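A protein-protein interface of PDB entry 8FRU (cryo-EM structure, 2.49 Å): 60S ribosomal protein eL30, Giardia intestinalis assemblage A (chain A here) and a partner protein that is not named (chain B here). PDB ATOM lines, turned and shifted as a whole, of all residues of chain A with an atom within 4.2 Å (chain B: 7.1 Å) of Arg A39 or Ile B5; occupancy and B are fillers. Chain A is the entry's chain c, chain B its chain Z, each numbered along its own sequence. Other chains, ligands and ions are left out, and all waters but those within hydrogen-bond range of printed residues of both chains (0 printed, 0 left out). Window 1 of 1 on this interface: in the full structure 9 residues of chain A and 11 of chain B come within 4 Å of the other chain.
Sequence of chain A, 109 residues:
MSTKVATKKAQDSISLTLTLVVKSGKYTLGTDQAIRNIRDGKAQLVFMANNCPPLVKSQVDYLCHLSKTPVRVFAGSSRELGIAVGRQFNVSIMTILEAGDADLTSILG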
ATOM      1  N   ILE A  35      26.761 -17.269 -12.465  1.00  0.00           N
ATOM      2  CA  ILE A  35      25.393 -17.673 -12.778  1.00  0.00           C
ATOM      3  C   ILE A  35      25.223 -19.178 -12.658  1.00  0.00           C
ATOM      4  O   ILE A  35      24.220 -19.656 -12.107  1.00  0.00           O
ATOM      5  CB  ILE A  35      24.987 -17.178 -14.177  1.00  0.00           C
ATOM      6  CG1 ILE A  35      24.986 -15.654 -14.220  1.00  0.00           C
ATOM      7  CG2 ILE A  35      23.635 -17.722 -14.557  1.00  0.00           C
ATOM      8  CD1 ILE A  35      24.257 -15.081 -15.411  1.00  0.00           C
ATOM      9  N   ARG A  36      26.193 -19.951 -13.144  1.00  0.00           N
ATOM     10  CA  ARG A  36      26.074 -21.401 -13.054  1.00  0.00           C
ATOM     11  C   ARG A  36      26.041 -21.867 -11.605  1.00  0.00           C
ATOM     12  O   ARG A  36      25.366 -22.848 -11.285  1.00  0.00           O
ATOM     13  CB  ARG A  36      27.211 -22.081 -13.813  1.00  0.00           C
ATOM     14  CG  ARG A  36      27.311 -21.680 -15.266  1.00  0.00           C
ATOM     15  CD  ARG A  36      27.956 -22.769 -16.100  1.00  0.00           C
ATOM     16  NE  ARG A  36      29.312 -23.075 -15.664  1.00  0.00           N
ATOM     17  CZ  ARG A  36      30.402 -22.513 -16.170  1.00  0.00           C
ATOM     18  NH1 ARG A  36      30.330 -21.576 -17.098  1.00  0.00           N
ATOM     19  NH2 ARG A  36      31.594 -22.898 -15.727  1.00  0.00           N
ATOM     20  N   ASN A  37      26.780 -21.198 -10.717  1.00  0.00           N
ATOM     21  CA  ASN A  37      26.756 -21.594  -9.312  1.00  0.00           C
ATOM     22  C   ASN A  37      25.465 -21.174  -8.618  1.00  0.00           C
ATOM     23  O   ASN A  37      24.861 -21.972  -7.897  1.00  0.00           O
ATOM     24  CB  ASN A  37      27.969 -21.027  -8.584  1.00  0.00           C
ATOM     25  CG  ASN A  37      29.261 -21.645  -9.055  1.00  0.00           C
ATOM     26  OD1 ASN A  37      30.290 -20.978  -9.138  1.00  0.00           O
ATOM     27  ND2 ASN A  37      29.214 -22.930  -9.375  1.00  0.00           N
ATOM     28  N   ILE A  38      25.015 -19.935  -8.823  1.00  0.00           N
ATOM     29  CA  ILE A  38      23.811 -19.472  -8.135  1.00  0.00           C
ATOM     30  C   ILE A  38      22.596 -20.285  -8.558  1.00  0.00           C
ATOM     31  O   ILE A  38      21.742 -20.623  -7.731  1.00  0.00           O
ATOM     32  CB  ILE A  38      23.589 -17.966  -8.359  1.00  0.00           C
ATOM     33  CG1 ILE A  38      24.917 -17.220  -8.390  1.00  0.00           C
ATOM     34  CG2 ILE A  38      22.708 -17.395  -7.281  1.00  0.00           C
ATOM     35  CD1 ILE A  38      24.847 -15.871  -9.078  1.00  0.00           C
ATOM     36  N   ARG A  39      22.485 -20.599  -9.851  1.00  0.00           N
ATOM     37  CA  ARG A  39      21.374 -21.432 -10.301  1.00  0.00           C
ATOM     38  C   ARG A  39      21.346 -22.775  -9.591  1.00  0.00           C
ATOM     39  O   ARG A  39      20.269 -23.342  -9.379  1.00  0.00           O
ATOM     40  CB  ARG A  39      21.465 -21.649 -11.806  1.00  0.00           C
ATOM     41  CG  ARG A  39      20.944 -20.521 -12.649  1.00  0.00           C
ATOM     42  CD  ARG A  39      21.097 -20.884 -14.107  1.00  0.00           C
ATOM     43  NE  ARG A  39      21.439 -22.290 -14.276  1.00  0.00           N
ATOM     44  CZ  ARG A  39      22.382 -22.724 -15.100  1.00  0.00           C
ATOM     45  NH1 ARG A  39      23.074 -21.891 -15.856  1.00  0.00           N
ATOM     46  NH2 ARG A  39      22.641 -24.026 -15.164  1.00  0.00           N
ATOM     47  N   ASP A  40      22.505 -23.297  -9.217  1.00  0.00           N
ATOM     48  CA  ASP A  40      22.605 -24.631  -8.649  1.00  0.00           C
ATOM     49  C   ASP A  40      22.485 -24.659  -7.131  1.00  0.00           C
ATOM     50  O   ASP A  40      22.523 -25.745  -6.547  1.00  0.00           O
ATOM     51  CB  ASP A  40      23.926 -25.274  -9.072  1.00  0.00           C
ATOM     52  CG  ASP A  40      23.791 -26.090 -10.336  1.00  0.00           C
ATOM     53  OD1 ASP A  40      22.958 -27.019 -10.355  1.00  0.00           O
ATOM     54  OD2 ASP A  40      24.501 -25.792 -11.320  1.00  0.00           O
ATOM     55  N   GLY A  41      22.337 -23.511  -6.480  1.00  0.00           N
ATOM     56  CA  GLY A  41      22.302 -23.478  -5.032  1.00  0.00           C
ATOM     57  C   GLY A  41      23.605 -23.921  -4.400  1.00  0.00           C
ATOM     58  O   GLY A  41      23.624 -24.816  -3.550  1.00  0.00           O
ATOM     59  N   LEU A  66      15.706 -15.348  -6.272  1.00  0.00           N
ATOM     60  CA  LEU A  66      15.014 -16.615  -6.461  1.00  0.00           C
ATOM     61  C   LEU A  66      15.711 -17.782  -5.778  1.00  0.00           C
ATOM     62  O   LEU A  66      15.102 -18.847  -5.641  1.00  0.00           O
ATOM     63  CB  LEU A  66      14.851 -16.923  -7.949  1.00  0.00           C
ATOM     64  CG  LEU A  66      13.630 -16.316  -8.633  1.00  0.00           C
ATOM     65  CD1 LEU A  66      13.696 -14.807  -8.578  1.00  0.00           C
ATOM     66  CD2 LEU A  66      13.549 -16.802 -10.066  1.00  0.00           C
ATOM     67  N   SER A  67      16.955 -17.616  -5.335  1.00  0.00           N
ATOM     68  CA  SER A  67      17.633 -18.691  -4.624  1.00  0.00           C
ATOM     69  C   SER A  67      17.941 -18.358  -3.170  1.00  0.00           C
ATOM     70  O   SER A  67      18.581 -19.167  -2.490  1.00  0.00           O
ATOM     71  CB  SER A  67      18.928 -19.078  -5.345  1.00  0.00           C
ATOM     72  OG  SER A  67      19.694 -17.931  -5.648  1.00  0.00           O
ATOM     73  N   GLN B   3      19.173 -22.675  -2.243  1.00  0.00           N
ATOM     74  CA  GLN B   3      18.334 -23.753  -2.732  1.00  0.00           C
ATOM     75  C   GLN B   3      18.298 -23.735  -4.253  1.00  0.00           C
ATOM     76  O   GLN B   3      18.075 -22.672  -4.849  1.00  0.00           O
ATOM     77  CB  GLN B   3      16.910 -23.633  -2.171  1.00  0.00           C
ATOM     78  N   PRO B   4      18.524 -24.868  -4.916  1.00  0.00           N
ATOM     79  CA  PRO B   4      18.435 -24.896  -6.382  1.00  0.00           C
ATOM     80  C   PRO B   4      17.058 -24.466  -6.861  1.00  0.00           C
ATOM     81  O   PRO B   4      16.041 -24.747  -6.226  1.00  0.00           O
ATOM     82  CB  PRO B   4      18.718 -26.361  -6.730  1.00  0.00           C
ATOM     83  CG  PRO B   4      18.559 -27.109  -5.446  1.00  0.00           C
ATOM     84  CD  PRO B   4      18.958 -26.160  -4.369  1.00  0.00           C
ATOM     85  N   ILE B   5      17.033 -23.773  -7.998  1.00  0.00           N
ATOM     86  CA  ILE B   5      15.795 -23.218  -8.534  1.00  0.00           C
ATOM     87  C   ILE B   5      15.291 -23.946  -9.770  1.00  0.00           C
ATOM     88  O   ILE B   5      14.154 -23.684 -10.195  1.00  0.00           O
ATOM     89  CB  ILE B   5      15.937 -21.712  -8.833  1.00  0.00           C
ATOM     90  CG1 ILE B   5      17.297 -21.423  -9.458  1.00  0.00           C
ATOM     91  CG2 ILE B   5      15.767 -20.907  -7.565  1.00  0.00           C
ATOM     92  CD1 ILE B   5      17.565 -19.961  -9.682  1.00  0.00           C
ATOM     93  N   ILE B   6      16.073 -24.846 -10.360  1.00  0.00           N
ATOM     94  CA  ILE B   6      15.654 -25.574 -11.555  1.00  0.00           C
ATOM     95  C   ILE B   6      14.966 -26.853 -11.091  1.00  0.00           C
ATOM     96  O   ILE B   6      15.621 -27.818 -10.697  1.00  0.00           O
ATOM     97  CB  ILE B   6      16.831 -25.869 -12.486  1.00  0.00           C
ATOM     98  CG1 ILE B   6      17.489 -24.567 -12.942  1.00  0.00           C
ATOM     99  CG2 ILE B   6      16.375 -26.694 -13.683  1.00  0.00           C
ATOM    100  CD1 ILE B   6      18.920 -24.739 -13.370  1.00  0.00           C
ATOM    101  N   LYS B   7      13.636 -26.858 -11.142  1.00  0.00           N
ATOM    102  CA  LYS B   7      12.830 -27.988 -10.707  1.00  0.00           C
ATOM    103  C   LYS B   7      11.621 -28.102 -11.619  1.00  0.00           C
ATOM    104  O   LYS B   7      11.192 -27.099 -12.198  1.00  0.00           O
ATOM    105  CB  LYS B   7      12.375 -27.822  -9.252  1.00  0.00           C
ATOM    106  CG  LYS B   7      11.790 -26.451  -8.944  1.00  0.00           C
ATOM    107  CD  LYS B   7      11.258 -26.382  -7.523  1.00  0.00           C
ATOM    108  CE  LYS B   7      12.175 -27.109  -6.554  1.00  0.00           C
ATOM    109  NZ  LYS B   7      13.506 -26.458  -6.438  1.00  0.00           N
ATOM    110  N   PRO B   8      11.050 -29.293 -11.762  1.00  0.00           N
ATOM    111  CA  PRO B   8       9.861 -29.435 -12.606  1.00  0.00           C
ATOM    112  C   PRO B   8       8.727 -28.544 -12.127  1.00  0.00           C
ATOM    113  O   PRO B   8       8.550 -28.319 -10.930  1.00  0.00           O
ATOM    114  CB  PRO B   8       9.510 -30.919 -12.470  1.00  0.00           C
ATOM    115  CG  PRO B   8      10.798 -31.567 -12.181  1.00  0.00           C
ATOM    116  CD  PRO B   8      11.573 -30.598 -11.332  1.00  0.00           C
ATOM    117  N   LEU B  10       8.478 -25.329 -13.085  1.00  0.00           N
ATOM    118  CA  LEU B  10       8.890 -23.940 -13.203  1.00  0.00           C
ATOM    119  C   LEU B  10       8.587 -23.396 -14.594  1.00  0.00           C
ATOM    120  O   LEU B  10       8.560 -24.132 -15.583  1.00  0.00           O
ATOM    121  CB  LEU B  10      10.381 -23.803 -12.906  1.00  0.00           C
ATOM    122  CG  LEU B  10      10.931 -22.381 -12.796  1.00  0.00           C
ATOM    123  CD1 LEU B  10      10.586 -21.775 -11.454  1.00  0.00           C
ATOM    124  CD2 LEU B  10      12.427 -22.380 -13.015  1.00  0.00           C
ATOM    125  N   ILE B  26       9.164 -26.480 -17.490  1.00  0.00           N
ATOM    126  CA  ILE B  26      10.122 -27.568 -17.342  1.00  0.00           C
ATOM    127  C   ILE B  26       9.406 -28.794 -16.796  1.00  0.00           C
ATOM    128  O   ILE B  26       8.713 -28.720 -15.775  1.00  0.00           O
ATOM    129  CB  ILE B  26      11.279 -27.150 -16.425  1.00  0.00           C
ATOM    130  CG1 ILE B  26      12.172 -26.138 -17.135  1.00  0.00           C
ATOM    131  CG2 ILE B  26      12.078 -28.362 -16.000  1.00  0.00           C
ATOM    132  CD1 ILE B  26      13.373 -25.721 -16.336  1.00  0.00           C
ATOM    133  N   SER B  37      24.307 -29.037 -18.745  1.00  0.00           N
ATOM    134  CA  SER B  37      23.014 -29.174 -18.085  1.00  0.00           C
ATOM    135  C   SER B  37      21.894 -29.010 -19.105  1.00  0.00           C
ATOM    136  O   SER B  37      21.809 -27.978 -19.775  1.00  0.00           O
ATOM    137  CB  SER B  37      22.860 -28.138 -16.973  1.00  0.00           C
ATOM    138  OG  SER B  37      24.096 -27.870 -16.340  1.00  0.00           O
ATOM    139  N   ASN B  74      19.476 -26.584 -23.615  1.00  0.00           N
ATOM    140  CA  ASN B  74      20.510 -26.135 -22.697  1.00  0.00           C
ATOM    141  C   ASN B  74      19.929 -25.248 -21.610  1.00  0.00           C
ATOM    142  O   ASN B  74      19.202 -24.295 -21.892  1.00  0.00           O
ATOM    143  CB  ASN B  74      21.574 -25.371 -23.477  1.00  0.00           C
ATOM    144  CG  ASN B  74      22.934 -25.457 -22.849  1.00  0.00           C
ATOM    145  OD1 ASN B  74      23.066 -25.482 -21.630  1.00  0.00           O
ATOM    146  ND2 ASN B  74      23.959 -25.496 -23.676  1.00  0.00           N
ATOM    147  N   VAL B  75      20.271 -25.551 -20.357  1.00  0.00           N
ATOM    148  CA  VAL B  75      19.772 -24.750 -19.250  1.00  0.00           C
ATOM    149  C   VAL B  75      20.357 -23.349 -19.262  1.00  0.00           C
ATOM    150  O   VAL B  75      19.785 -22.438 -18.657  1.00  0.00           O
ATOM    151  CB  VAL B  75      20.050 -25.454 -17.911  1.00  0.00           C
ATOM    152  CG1 VAL B  75      19.690 -24.547 -16.754  1.00  0.00           C
ATOM    153  CG2 VAL B  75      19.259 -26.740 -17.831  1.00  0.00           C
ATOM    154  N   ASN B  76      21.488 -23.148 -19.939  1.00  0.00           N
ATOM    155  CA  ASN B  76      22.035 -21.806 -20.082  1.00  0.00           C
ATOM    156  C   ASN B  76      21.160 -20.912 -20.949  1.00  0.00           C
ATOM    157  O   ASN B  76      21.288 -19.687 -20.878  1.00  0.00           O
ATOM    158  CB  ASN B  76      23.442 -21.874 -20.669  1.00  0.00           C
ATOM    159  CG  ASN B  76      24.483 -22.254 -19.642  1.00  0.00           C
ATOM    160  OD1 ASN B  76      24.322 -21.995 -18.453  1.00  0.00           O
ATOM    161  ND2 ASN B  76      25.556 -22.881 -20.096  1.00  0.00           N
ATOM    162  N   HIS B  77      20.277 -21.493 -21.757  1.00  0.00           N
ATOM    163  CA  HIS B  77      19.456 -20.748 -22.699  1.00  0.00           C
ATOM    164  C   HIS B  77      18.079 -20.414 -22.141  1.00  0.00           C
ATOM    165  O   HIS B  77      17.178 -20.060 -22.907  1.00  0.00           O
ATOM    166  CB  HIS B  77      19.313 -21.530 -24.005  1.00  0.00           C
ATOM    167  CG  HIS B  77      20.605 -21.752 -24.726  1.00  0.00           C
ATOM    168  ND1 HIS B  77      20.772 -22.753 -25.657  1.00  0.00           N
ATOM    169  CD2 HIS B  77      21.787 -21.102 -24.658  1.00  0.00           C
ATOM    170  CE1 HIS B  77      22.004 -22.712 -26.128  1.00  0.00           C
ATOM    171  NE2 HIS B  77      22.641 -21.718 -25.540  1.00  0.00           N
ATOM    172  N   LEU B  78      17.890 -20.520 -20.830  1.00  0.00           N
ATOM    173  CA  LEU B  78      16.602 -20.277 -20.204  1.00  0.00           C
ATOM    174  C   LEU B  78      16.716 -19.183 -19.154  1.00  0.00           C
ATOM    175  O   LEU B  78      17.782 -18.955 -18.580  1.00  0.00           O
ATOM    176  CB  LEU B  78      16.049 -21.550 -19.563  1.00  0.00           C
ATOM    177  CG  LEU B  78      15.885 -22.737 -20.510  1.00  0.00           C
ATOM    178  CD1 LEU B  78      15.781 -24.034 -19.735  1.00  0.00           C
ATOM    179  CD2 LEU B  78      14.684 -22.548 -21.415  1.00  0.00           C
ATOM    180  N   PRO B  80      14.766 -18.531 -15.735  1.00  0.00           N
ATOM    181  CA  PRO B  80      13.752 -18.961 -14.767  1.00  0.00           C
ATOM    182  C   PRO B  80      12.978 -17.778 -14.209  1.00  0.00           C
ATOM    183  O   PRO B  80      13.498 -16.669 -14.088  1.00  0.00           O
ATOM    184  CB  PRO B  80      14.573 -19.660 -13.679  1.00  0.00           C
ATOM    185  CG  PRO B  80      15.939 -19.111 -13.822  1.00  0.00           C
ATOM    186  CD  PRO B  80      16.135 -18.785 -15.262  1.00  0.00           C
ATOM    187  N   THR B  81      11.718 -18.025 -13.870  1.00  0.00           N
ATOM    188  CA  THR B  81      10.799 -16.993 -13.411  1.00  0.00           C
ATOM    189  C   THR B  81      10.223 -17.369 -12.049  1.00  0.00           C
ATOM    190  O   THR B  81      10.572 -18.392 -11.456  1.00  0.00           O
ATOM    191  CB  THR B  81       9.668 -16.773 -14.418  1.00  0.00           C
ATOM    192  OG1 THR B  81       8.965 -18.005 -14.620  1.00  0.00           O
ATOM    193  CG2 THR B  81      10.222 -16.300 -15.743  1.00  0.00           C
ATOM    194  N   ARG B  84       4.546 -20.635 -11.673  1.00  0.00           N
ATOM    195  CA  ARG B  84       4.430 -22.084 -11.614  1.00  0.00           C
ATOM    196  C   ARG B  84       3.293 -22.532 -12.520  1.00  0.00           C
ATOM    197  O   ARG B  84       2.386 -21.762 -12.837  1.00  0.00           O
ATOM    198  CB  ARG B  84       4.192 -22.576 -10.182  1.00  0.00           C
ATOM    199  CG  ARG B  84       5.455 -22.923  -9.420  1.00  0.00           C
ATOM    200  CD  ARG B  84       5.191 -24.004  -8.391  1.00  0.00           C
ATOM    201  NE  ARG B  84       5.445 -25.339  -8.915  1.00  0.00           N
ATOM    202  CZ  ARG B  84       6.652 -25.840  -9.136  1.00  0.00           C
ATOM    203  NH1 ARG B  84       7.746 -25.142  -8.883  1.00  0.00           N
ATOM    204  NH2 ARG B  84       6.766 -27.071  -9.622  1.00  0.00           N
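Among the printed residues, merely in contact across the chains: Arg A39 with Pro B4, Arg A39 with Ile B5, Arg A39 with Ile B6, Arg A39 with Val B75, Asp A40 with Pro B4, Leu A66 with Ile B5, Leu A66 with Thr B81 and Ser A67 with Gln B3.
The side-chain amino group (NZ) of Lys B7 lies within hydrogen-bond range of the backbone carbonyl oxygen (O) of Pro B4.
The backbone carbonyl oxygen (O) of Ser B37 sits at hydrogen-bond distance from the backbone NH (N) of Val B75 (2.9 Å).
The backbone NH (N) of Asn B76 sits close to the side-chain amide oxygen (OD1) of Asn B74 (3.3 Å).
Of the printed residues of chain A, Val B75 touches Arg A39 (3.4 Å).
Of the printed residues of chain B, Leu A66 touches Ile B5 and Thr B81.
Of the printed residues of chain A, Thr B81 touches Leu A66 (3.7 Å).
Of the printed residues of chain A, Gln B3 touches Ser A67 (3.6 Å).
Of the printed residues of chain A, Pro B4 touches Arg A39 and Asp A40.
Arg A36 touches none of the printed residues of chain B.
The nearest residue of chain B that does not touch Arg A39 is Ser B37 (4.3 Å).
The nearest residue of chain A that does not touch Ile B5 is Ser A67 (4.1 Å).
The nearest printed residue of chain A that does not touch Ile B6 is Asp A40 (5.5 Å).
Printed residues of chain B that touch a printed residue of chain A: Gln B3, Pro B4, Ile B5, Ile B6, Val B75, Asn B76 and Thr B81.
Hydrophobic or aromatic side chains of chain B within 4 Å of the printed part of chain A: Pro B4, Ile B5, Ile B6 and Val B75.
Of the 9 printed residues of chain A, 4 touch a printed residue of chain B.
Printed residues of chain A that touch a printed residue of chain B: Arg A39, Asp A40, Leu A66 and Ser A67.
The guanidinium group of Arg A39 sits at hydrogen-bond distance from the side-chain amide oxygen of Asn B76.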
